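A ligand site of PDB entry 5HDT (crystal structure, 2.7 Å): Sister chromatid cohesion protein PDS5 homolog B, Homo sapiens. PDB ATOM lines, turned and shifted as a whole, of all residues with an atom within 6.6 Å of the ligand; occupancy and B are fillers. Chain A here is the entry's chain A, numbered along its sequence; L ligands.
Merely in contact with the ligand: Tyr 719 (3.8 Å) and Gln 818 (3.99 Å).
The nearest printed residue that does not touch the ligand is Gln 681 (4.3 Å).
OH of Tyr 719 lies within hydrogen-bond range of NH1 of Arg 715 (3.3 Å).
The side-chain hydroxyl (OH) of Tyr 719 sits at hydrogen-bond distance from the side-chain amide oxygen (OE1) of Gln 681, at 3.5 Å.
The guanidinium group (NH2) of Arg 715 lies within salt-bridge range of an oxygen (O22) of the ligand (2.4 Å).
An oxygen (O23) of the ligand is in salt-bridge range of the side-chain amino group of Lys 718 (2.6 Å).
The guanidinium group (NH2) of Arg 825 lies within salt-bridge range of an oxygen (O18) of the ligand, at 2.7 Å.
O19 of the ligand is in salt-bridge range of NZ of Lys 821 (2.8 Å).
O10 of the ligand is in salt-bridge range of NZ of Lys 919.
The guanidinium group of Arg 923 is in salt-bridge range of an oxygen (O6) of the ligand.
NZ of Lys 916 lies within salt-bridge range of O16 of the ligand (3.1 Å).
NZ of Lys 879 lies within salt-bridge range of O11 of the ligand, 3.9 Å away.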
ATOM      1  N   GLN A 681      29.857  15.998  20.506  1.00  0.00           N
ATOM      2  CA  GLN A 681      30.362  15.969  21.874  1.00  0.00           C
ATOM      3  C   GLN A 681      30.884  17.339  22.301  1.00  0.00           C
ATOM      4  O   GLN A 681      30.771  17.726  23.456  1.00  0.00           O
ATOM      5  CB  GLN A 681      31.454  14.913  22.019  1.00  0.00           C
ATOM      6  CG  GLN A 681      31.918  14.694  23.455  1.00  0.00           C
ATOM      7  CD  GLN A 681      32.504  13.316  23.686  1.00  0.00           C
ATOM      8  OE1 GLN A 681      32.835  12.600  22.731  1.00  0.00           O
ATOM      9  NE2 GLN A 681      32.617  12.917  24.948  1.00  0.00           N
ATOM     10  N   LYS A 684      27.859  19.683  22.933  1.00  0.00           N
ATOM     11  CA  LYS A 684      27.307  19.307  24.234  1.00  0.00           C
ATOM     12  C   LYS A 684      28.050  19.994  25.375  1.00  0.00           C
ATOM     13  O   LYS A 684      27.445  20.361  26.383  1.00  0.00           O
ATOM     14  CB  LYS A 684      27.364  17.781  24.398  1.00  0.00           C
ATOM     15  CG  LYS A 684      27.182  17.274  25.820  1.00  0.00           C
ATOM     16  CD  LYS A 684      27.231  15.753  25.844  1.00  0.00           C
ATOM     17  CE  LYS A 684      27.250  15.218  27.262  1.00  0.00           C
ATOM     18  NZ  LYS A 684      27.320  13.722  27.288  1.00  0.00           N
ATOM     19  N   PRO A 714      23.689   5.173  16.896  1.00  0.00           N
ATOM     20  CA  PRO A 714      23.440   5.226  18.339  1.00  0.00           C
ATOM     21  C   PRO A 714      24.300   6.243  19.073  1.00  0.00           C
ATOM     22  O   PRO A 714      23.754   7.076  19.798  1.00  0.00           O
ATOM     23  CB  PRO A 714      23.780   3.803  18.795  1.00  0.00           C
ATOM     24  CG  PRO A 714      23.528   2.960  17.612  1.00  0.00           C
ATOM     25  CD  PRO A 714      23.916   3.790  16.428  1.00  0.00           C
ATOM     26  N   ARG A 715      25.613   6.183  18.887  1.00  0.00           N
ATOM     27  CA  ARG A 715      26.534   7.083  19.567  1.00  0.00           C
ATOM     28  C   ARG A 715      26.156   8.541  19.326  1.00  0.00           C
ATOM     29  O   ARG A 715      26.113   9.352  20.244  1.00  0.00           O
ATOM     30  CB  ARG A 715      27.970   6.824  19.120  1.00  0.00           C
ATOM     31  CG  ARG A 715      29.039   7.228  20.140  1.00  0.00           C
ATOM     32  CD  ARG A 715      30.410   6.682  19.757  1.00  0.00           C
ATOM     33  NE  ARG A 715      31.316   6.583  20.899  1.00  0.00           N
ATOM     34  CZ  ARG A 715      32.155   7.531  21.287  1.00  0.00           C
ATOM     35  NH1 ARG A 715      32.239   8.683  20.629  1.00  0.00           N
ATOM     36  NH2 ARG A 715      32.934   7.330  22.351  1.00  0.00           N
ATOM     37  N   LYS A 718      22.768   9.538  20.992  1.00  0.00           N
ATOM     38  CA  LYS A 718      22.966   9.864  22.402  1.00  0.00           C
ATOM     39  C   LYS A 718      23.428  11.296  22.574  1.00  0.00           C
ATOM     40  O   LYS A 718      22.813  12.081  23.306  1.00  0.00           O
ATOM     41  CB  LYS A 718      23.983   8.902  23.022  1.00  0.00           C
ATOM     42  CG  LYS A 718      24.570   9.372  24.336  1.00  0.00           C
ATOM     43  CD  LYS A 718      25.458   8.312  24.962  1.00  0.00           C
ATOM     44  CE  LYS A 718      26.740   8.134  24.158  1.00  0.00           C
ATOM     45  NZ  LYS A 718      27.588   7.097  24.757  1.00  0.00           N
ATOM     46  N   TYR A 719      24.528  11.644  21.909  1.00  0.00           N
ATOM     47  CA  TYR A 719      25.094  12.984  22.010  1.00  0.00           C
ATOM     48  C   TYR A 719      24.085  14.034  21.538  1.00  0.00           C
ATOM     49  O   TYR A 719      24.024  15.123  22.100  1.00  0.00           O
ATOM     50  CB  TYR A 719      26.385  13.080  21.186  1.00  0.00           C
ATOM     51  CG  TYR A 719      27.527  12.240  21.729  1.00  0.00           C
ATOM     52  CD1 TYR A 719      27.687  12.030  23.092  1.00  0.00           C
ATOM     53  CD2 TYR A 719      28.446  11.645  20.865  1.00  0.00           C
ATOM     54  CE1 TYR A 719      28.718  11.268  23.590  1.00  0.00           C
ATOM     55  CE2 TYR A 719      29.481  10.876  21.357  1.00  0.00           C
ATOM     56  CZ  TYR A 719      29.615  10.691  22.723  1.00  0.00           C
ATOM     57  OH  TYR A 719      30.649   9.931  23.203  1.00  0.00           O
ATOM     58  N   VAL A 759      18.227   3.538  22.534  1.00  0.00           N
ATOM     59  CA  VAL A 759      19.253   4.446  23.032  1.00  0.00           C
ATOM     60  C   VAL A 759      18.665   5.828  23.286  1.00  0.00           C
ATOM     61  O   VAL A 759      18.806   6.391  24.362  1.00  0.00           O
ATOM     62  CB  VAL A 759      20.436   4.557  22.050  1.00  0.00           C
ATOM     63  CG1 VAL A 759      21.409   5.654  22.479  1.00  0.00           C
ATOM     64  CG2 VAL A 759      21.174   3.221  21.947  1.00  0.00           C
ATOM     65  N   HIS A 763      18.088   7.903  27.019  1.00  0.00           N
ATOM     66  CA  HIS A 763      18.689   9.171  27.421  1.00  0.00           C
ATOM     67  C   HIS A 763      17.625  10.225  27.666  1.00  0.00           C
ATOM     68  O   HIS A 763      17.818  11.138  28.476  1.00  0.00           O
ATOM     69  CB  HIS A 763      19.686   9.634  26.363  1.00  0.00           C
ATOM     70  CG  HIS A 763      20.927   8.804  26.316  1.00  0.00           C
ATOM     71  ND1 HIS A 763      21.932   8.911  27.251  1.00  0.00           N
ATOM     72  CD2 HIS A 763      21.330   7.835  25.453  1.00  0.00           C
ATOM     73  CE1 HIS A 763      22.895   8.064  26.969  1.00  0.00           C
ATOM     74  NE2 HIS A 763      22.553   7.401  25.880  1.00  0.00           N
ATOM     75  N   GLN A 818      20.811  -3.460  25.265  1.00  0.00           N
ATOM     76  CA  GLN A 818      20.481  -2.053  25.145  1.00  0.00           C
ATOM     77  C   GLN A 818      19.181  -1.742  25.890  1.00  0.00           C
ATOM     78  O   GLN A 818      18.972  -0.619  26.344  1.00  0.00           O
ATOM     79  CB  GLN A 818      20.366  -1.643  23.685  1.00  0.00           C
ATOM     80  CG  GLN A 818      20.788  -0.213  23.409  1.00  0.00           C
ATOM     81  CD  GLN A 818      22.255   0.023  23.673  1.00  0.00           C
ATOM     82  OE1 GLN A 818      23.113  -0.662  23.133  1.00  0.00           O
ATOM     83  NE2 GLN A 818      22.554   0.986  24.539  1.00  0.00           N
ATOM     84  N   LYS A 821      20.265  -1.434  29.575  1.00  0.00           N
ATOM     85  CA  LYS A 821      20.889  -0.136  29.777  1.00  0.00           C
ATOM     86  C   LYS A 821      19.830   0.969  29.776  1.00  0.00           C
ATOM     87  O   LYS A 821      19.993   2.001  30.427  1.00  0.00           O
ATOM     88  CB  LYS A 821      21.950   0.154  28.701  1.00  0.00           C
ATOM     89  CG  LYS A 821      23.119  -0.831  28.706  1.00  0.00           C
ATOM     90  CD  LYS A 821      24.393  -0.222  28.115  1.00  0.00           C
ATOM     91  CE  LYS A 821      25.065   0.725  29.100  1.00  0.00           C
ATOM     92  NZ  LYS A 821      26.324   1.324  28.547  1.00  0.00           N
ATOM     93  N   ARG A 825      18.979   3.756  32.915  1.00  0.00           N
ATOM     94  CA  ARG A 825      18.885   5.188  32.680  1.00  0.00           C
ATOM     95  C   ARG A 825      17.505   5.696  33.086  1.00  0.00           C
ATOM     96  O   ARG A 825      17.363   6.814  33.564  1.00  0.00           O
ATOM     97  CB  ARG A 825      19.166   5.501  31.206  1.00  0.00           C
ATOM     98  CG  ARG A 825      20.613   5.241  30.803  1.00  0.00           C
ATOM     99  CD  ARG A 825      20.923   5.729  29.401  1.00  0.00           C
ATOM    100  NE  ARG A 825      22.326   5.532  29.065  1.00  0.00           N
ATOM    101  CZ  ARG A 825      22.807   4.529  28.326  1.00  0.00           C
ATOM    102  NH1 ARG A 825      22.011   3.596  27.826  1.00  0.00           N
ATOM    103  NH2 ARG A 825      24.118   4.455  28.085  1.00  0.00           N
ATOM    104  N   LYS A 879      25.959  -0.167  38.537  1.00  0.00           N
ATOM    105  CA  LYS A 879      25.709   1.212  38.154  1.00  0.00           C
ATOM    106  C   LYS A 879      24.620   1.829  39.035  1.00  0.00           C
ATOM    107  O   LYS A 879      24.721   2.996  39.425  1.00  0.00           O
ATOM    108  CB  LYS A 879      25.296   1.306  36.684  1.00  0.00           C
ATOM    109  CG  LYS A 879      25.584   2.663  36.050  1.00  0.00           C
ATOM    110  CD  LYS A 879      24.933   2.784  34.683  1.00  0.00           C
ATOM    111  CE  LYS A 879      25.507   3.934  33.888  1.00  0.00           C
ATOM    112  NZ  LYS A 879      24.799   4.112  32.583  1.00  0.00           N
ATOM    113  N   GLN A 882      25.700   2.861  42.528  1.00  0.00           N
ATOM    114  CA  GLN A 882      26.391   4.143  42.602  1.00  0.00           C
ATOM    115  C   GLN A 882      25.418   5.297  42.808  1.00  0.00           C
ATOM    116  O   GLN A 882      25.833   6.439  42.989  1.00  0.00           O
ATOM    117  CB  GLN A 882      27.233   4.373  41.338  1.00  0.00           C
ATOM    118  CG  GLN A 882      28.374   3.390  41.192  1.00  0.00           C
ATOM    119  CD  GLN A 882      29.121   3.552  39.886  1.00  0.00           C
ATOM    120  OE1 GLN A 882      29.303   4.655  39.386  1.00  0.00           O
ATOM    121  NE2 GLN A 882      29.545   2.428  39.313  1.00  0.00           N
ATOM    122  N   VAL A 912      35.468  -7.635  32.405  1.00  0.00           N
ATOM    123  CA  VAL A 912      34.730  -6.394  32.230  1.00  0.00           C
ATOM    124  C   VAL A 912      33.974  -6.004  33.507  1.00  0.00           C
ATOM    125  O   VAL A 912      33.883  -4.824  33.835  1.00  0.00           O
ATOM    126  CB  VAL A 912      33.733  -6.488  31.065  1.00  0.00           C
ATOM    127  CG1 VAL A 912      32.918  -5.207  30.940  1.00  0.00           C
ATOM    128  CG2 VAL A 912      34.472  -6.758  29.765  1.00  0.00           C
ATOM    129  N   LYS A 916      34.358  -2.518  35.724  1.00  0.00           N
ATOM    130  CA  LYS A 916      33.251  -1.668  36.143  1.00  0.00           C
ATOM    131  C   LYS A 916      33.325  -1.363  37.627  1.00  0.00           C
ATOM    132  O   LYS A 916      33.001  -0.250  38.057  1.00  0.00           O
ATOM    133  CB  LYS A 916      31.914  -2.336  35.795  1.00  0.00           C
ATOM    134  CG  LYS A 916      31.595  -2.355  34.310  1.00  0.00           C
ATOM    135  CD  LYS A 916      31.086  -1.007  33.833  1.00  0.00           C
ATOM    136  CE  LYS A 916      30.948  -0.961  32.317  1.00  0.00           C
ATOM    137  NZ  LYS A 916      32.244  -0.677  31.655  1.00  0.00           N
ATOM    138  N   LYS A 919      36.125   1.237  38.151  1.00  0.00           N
ATOM    139  CA  LYS A 919      35.688   2.561  37.727  1.00  0.00           C
ATOM    140  C   LYS A 919      34.770   3.197  38.774  1.00  0.00           C
ATOM    141  O   LYS A 919      34.899   4.378  39.076  1.00  0.00           O
ATOM    142  CB  LYS A 919      34.984   2.486  36.370  1.00  0.00           C
ATOM    143  CG  LYS A 919      34.660   3.839  35.762  1.00  0.00           C
ATOM    144  CD  LYS A 919      34.326   3.735  34.283  1.00  0.00           C
ATOM    145  CE  LYS A 919      33.028   2.970  34.038  1.00  0.00           C
ATOM    146  NZ  LYS A 919      32.747   2.804  32.592  1.00  0.00           N
ATOM    147  N   ARG A 923      35.996   6.577  41.236  1.00  0.00           N
ATOM    148  CA  ARG A 923      35.257   7.828  41.266  1.00  0.00           C
ATOM    149  C   ARG A 923      34.646   8.078  42.638  1.00  0.00           C
ATOM    150  O   ARG A 923      33.910   9.042  42.822  1.00  0.00           O
ATOM    151  CB  ARG A 923      34.174   7.807  40.192  1.00  0.00           C
ATOM    152  CG  ARG A 923      34.724   7.656  38.789  1.00  0.00           C
ATOM    153  CD  ARG A 923      33.619   7.473  37.761  1.00  0.00           C
ATOM    154  NE  ARG A 923      34.148   7.485  36.403  1.00  0.00           N
ATOM    155  CZ  ARG A 923      33.414   7.288  35.308  1.00  0.00           C
ATOM    156  NH1 ARG A 923      32.118   7.047  35.405  1.00  0.00           N
ATOM    157  NH2 ARG A 923      33.991   7.316  34.113  1.00  0.00           N
ATOM    158  N   ARG A 925      32.264   6.665  44.150  1.00  0.00           N
ATOM    159  CA  ARG A 925      30.804   6.639  44.092  1.00  0.00           C
ATOM    160  C   ARG A 925      30.255   5.253  44.393  1.00  0.00           C
ATOM    161  O   ARG A 925      29.049   5.078  44.550  1.00  0.00           O
ATOM    162  CB  ARG A 925      30.312   7.106  42.714  1.00  0.00           C
ATOM    163  CG  ARG A 925      30.598   8.570  42.430  1.00  0.00           C
ATOM    164  CD  ARG A 925      29.750   9.121  41.296  1.00  0.00           C
ATOM    165  NE  ARG A 925      30.015   8.454  40.023  1.00  0.00           N
ATOM    166  CZ  ARG A 925      29.162   7.672  39.354  1.00  0.00           C
ATOM    167  NH1 ARG A 925      27.939   7.432  39.817  1.00  0.00           N
ATOM    168  NH2 ARG A 925      29.538   7.132  38.205  1.00  0.00           N
HETATM  169  C1  LIG L   1      29.486   6.118  27.939  1.00  0.00           C
HETATM  170  C2  LIG L   1      29.667   5.541  29.341  1.00  0.00           C
HETATM  171  C3  LIG L   1      29.410   4.047  29.540  1.00  0.00           C
HETATM  172  C4  LIG L   1      29.837   3.168  28.397  1.00  0.00           C
HETATM  173  C5  LIG L   1      29.217   3.758  27.158  1.00  0.00           C
HETATM  174  C6  LIG L   1      29.560   5.172  26.747  1.00  0.00           C
HETATM  175  O1  LIG L   1      30.459   7.131  27.732  1.00  0.00           O
HETATM  176  P1  LIG L   1      29.922   8.625  27.662  1.00  0.00           P
HETATM  177  O2  LIG L   1      28.655   8.671  26.829  1.00  0.00           O
HETATM  178  O3  LIG L   1      30.961   9.532  27.026  1.00  0.00           O
HETATM  179  O4  LIG L   1      29.611   9.104  29.050  1.00  0.00           O
HETATM  180  O5  LIG L   1      30.996   5.856  29.809  1.00  0.00           O
HETATM  181  P2  LIG L   1      31.177   6.644  31.173  1.00  0.00           P
HETATM  182  O6  LIG L   1      32.343   6.046  31.930  1.00  0.00           O
HETATM  183  O7  LIG L   1      31.484   8.099  30.882  1.00  0.00           O
HETATM  184  O8  LIG L   1      29.933   6.565  32.029  1.00  0.00           O
HETATM  185  O9  LIG L   1      30.063   3.584  30.715  1.00  0.00           O
HETATM  186  P3  LIG L   1      29.179   3.031  31.908  1.00  0.00           P
HETATM  187  O10 LIG L   1      30.015   2.114  32.761  1.00  0.00           O
HETATM  188  O11 LIG L   1      27.971   2.280  31.389  1.00  0.00           O
HETATM  189  O12 LIG L   1      28.693   4.186  32.755  1.00  0.00           O
HETATM  190  O13 LIG L   1      29.334   1.843  28.620  1.00  0.00           O
HETATM  191  P4  LIG L   1      30.073   0.525  28.039  1.00  0.00           P
HETATM  192  O14 LIG L   1      30.540   0.749  26.612  1.00  0.00           O
HETATM  193  O15 LIG L   1      29.087  -0.629  28.074  1.00  0.00           O
HETATM  194  O16 LIG L   1      31.258   0.186  28.897  1.00  0.00           O
HETATM  195  O17 LIG L   1      28.428   2.950  26.282  1.00  0.00           O
HETATM  196  P5  LIG L   1      26.993   3.483  25.940  1.00  0.00           P
HETATM  197  O18 LIG L   1      26.581   4.559  26.931  1.00  0.00           O
HETATM  198  O19 LIG L   1      26.007   2.346  26.006  1.00  0.00           O
HETATM  199  O20 LIG L   1      27.024   4.073  24.547  1.00  0.00           O
HETATM  200  O21 LIG L   1      30.852   5.232  26.153  1.00  0.00           O
HETATM  201  P6  LIG L   1      31.056   5.568  24.644  1.00  0.00           P
HETATM  202  O22 LIG L   1      32.115   6.637  24.524  1.00  0.00           O
HETATM  203  O23 LIG L   1      29.797   6.052  23.978  1.00  0.00           O
HETATM  204  O24 LIG L   1      31.521   4.319  23.939  1.00  0.00           O
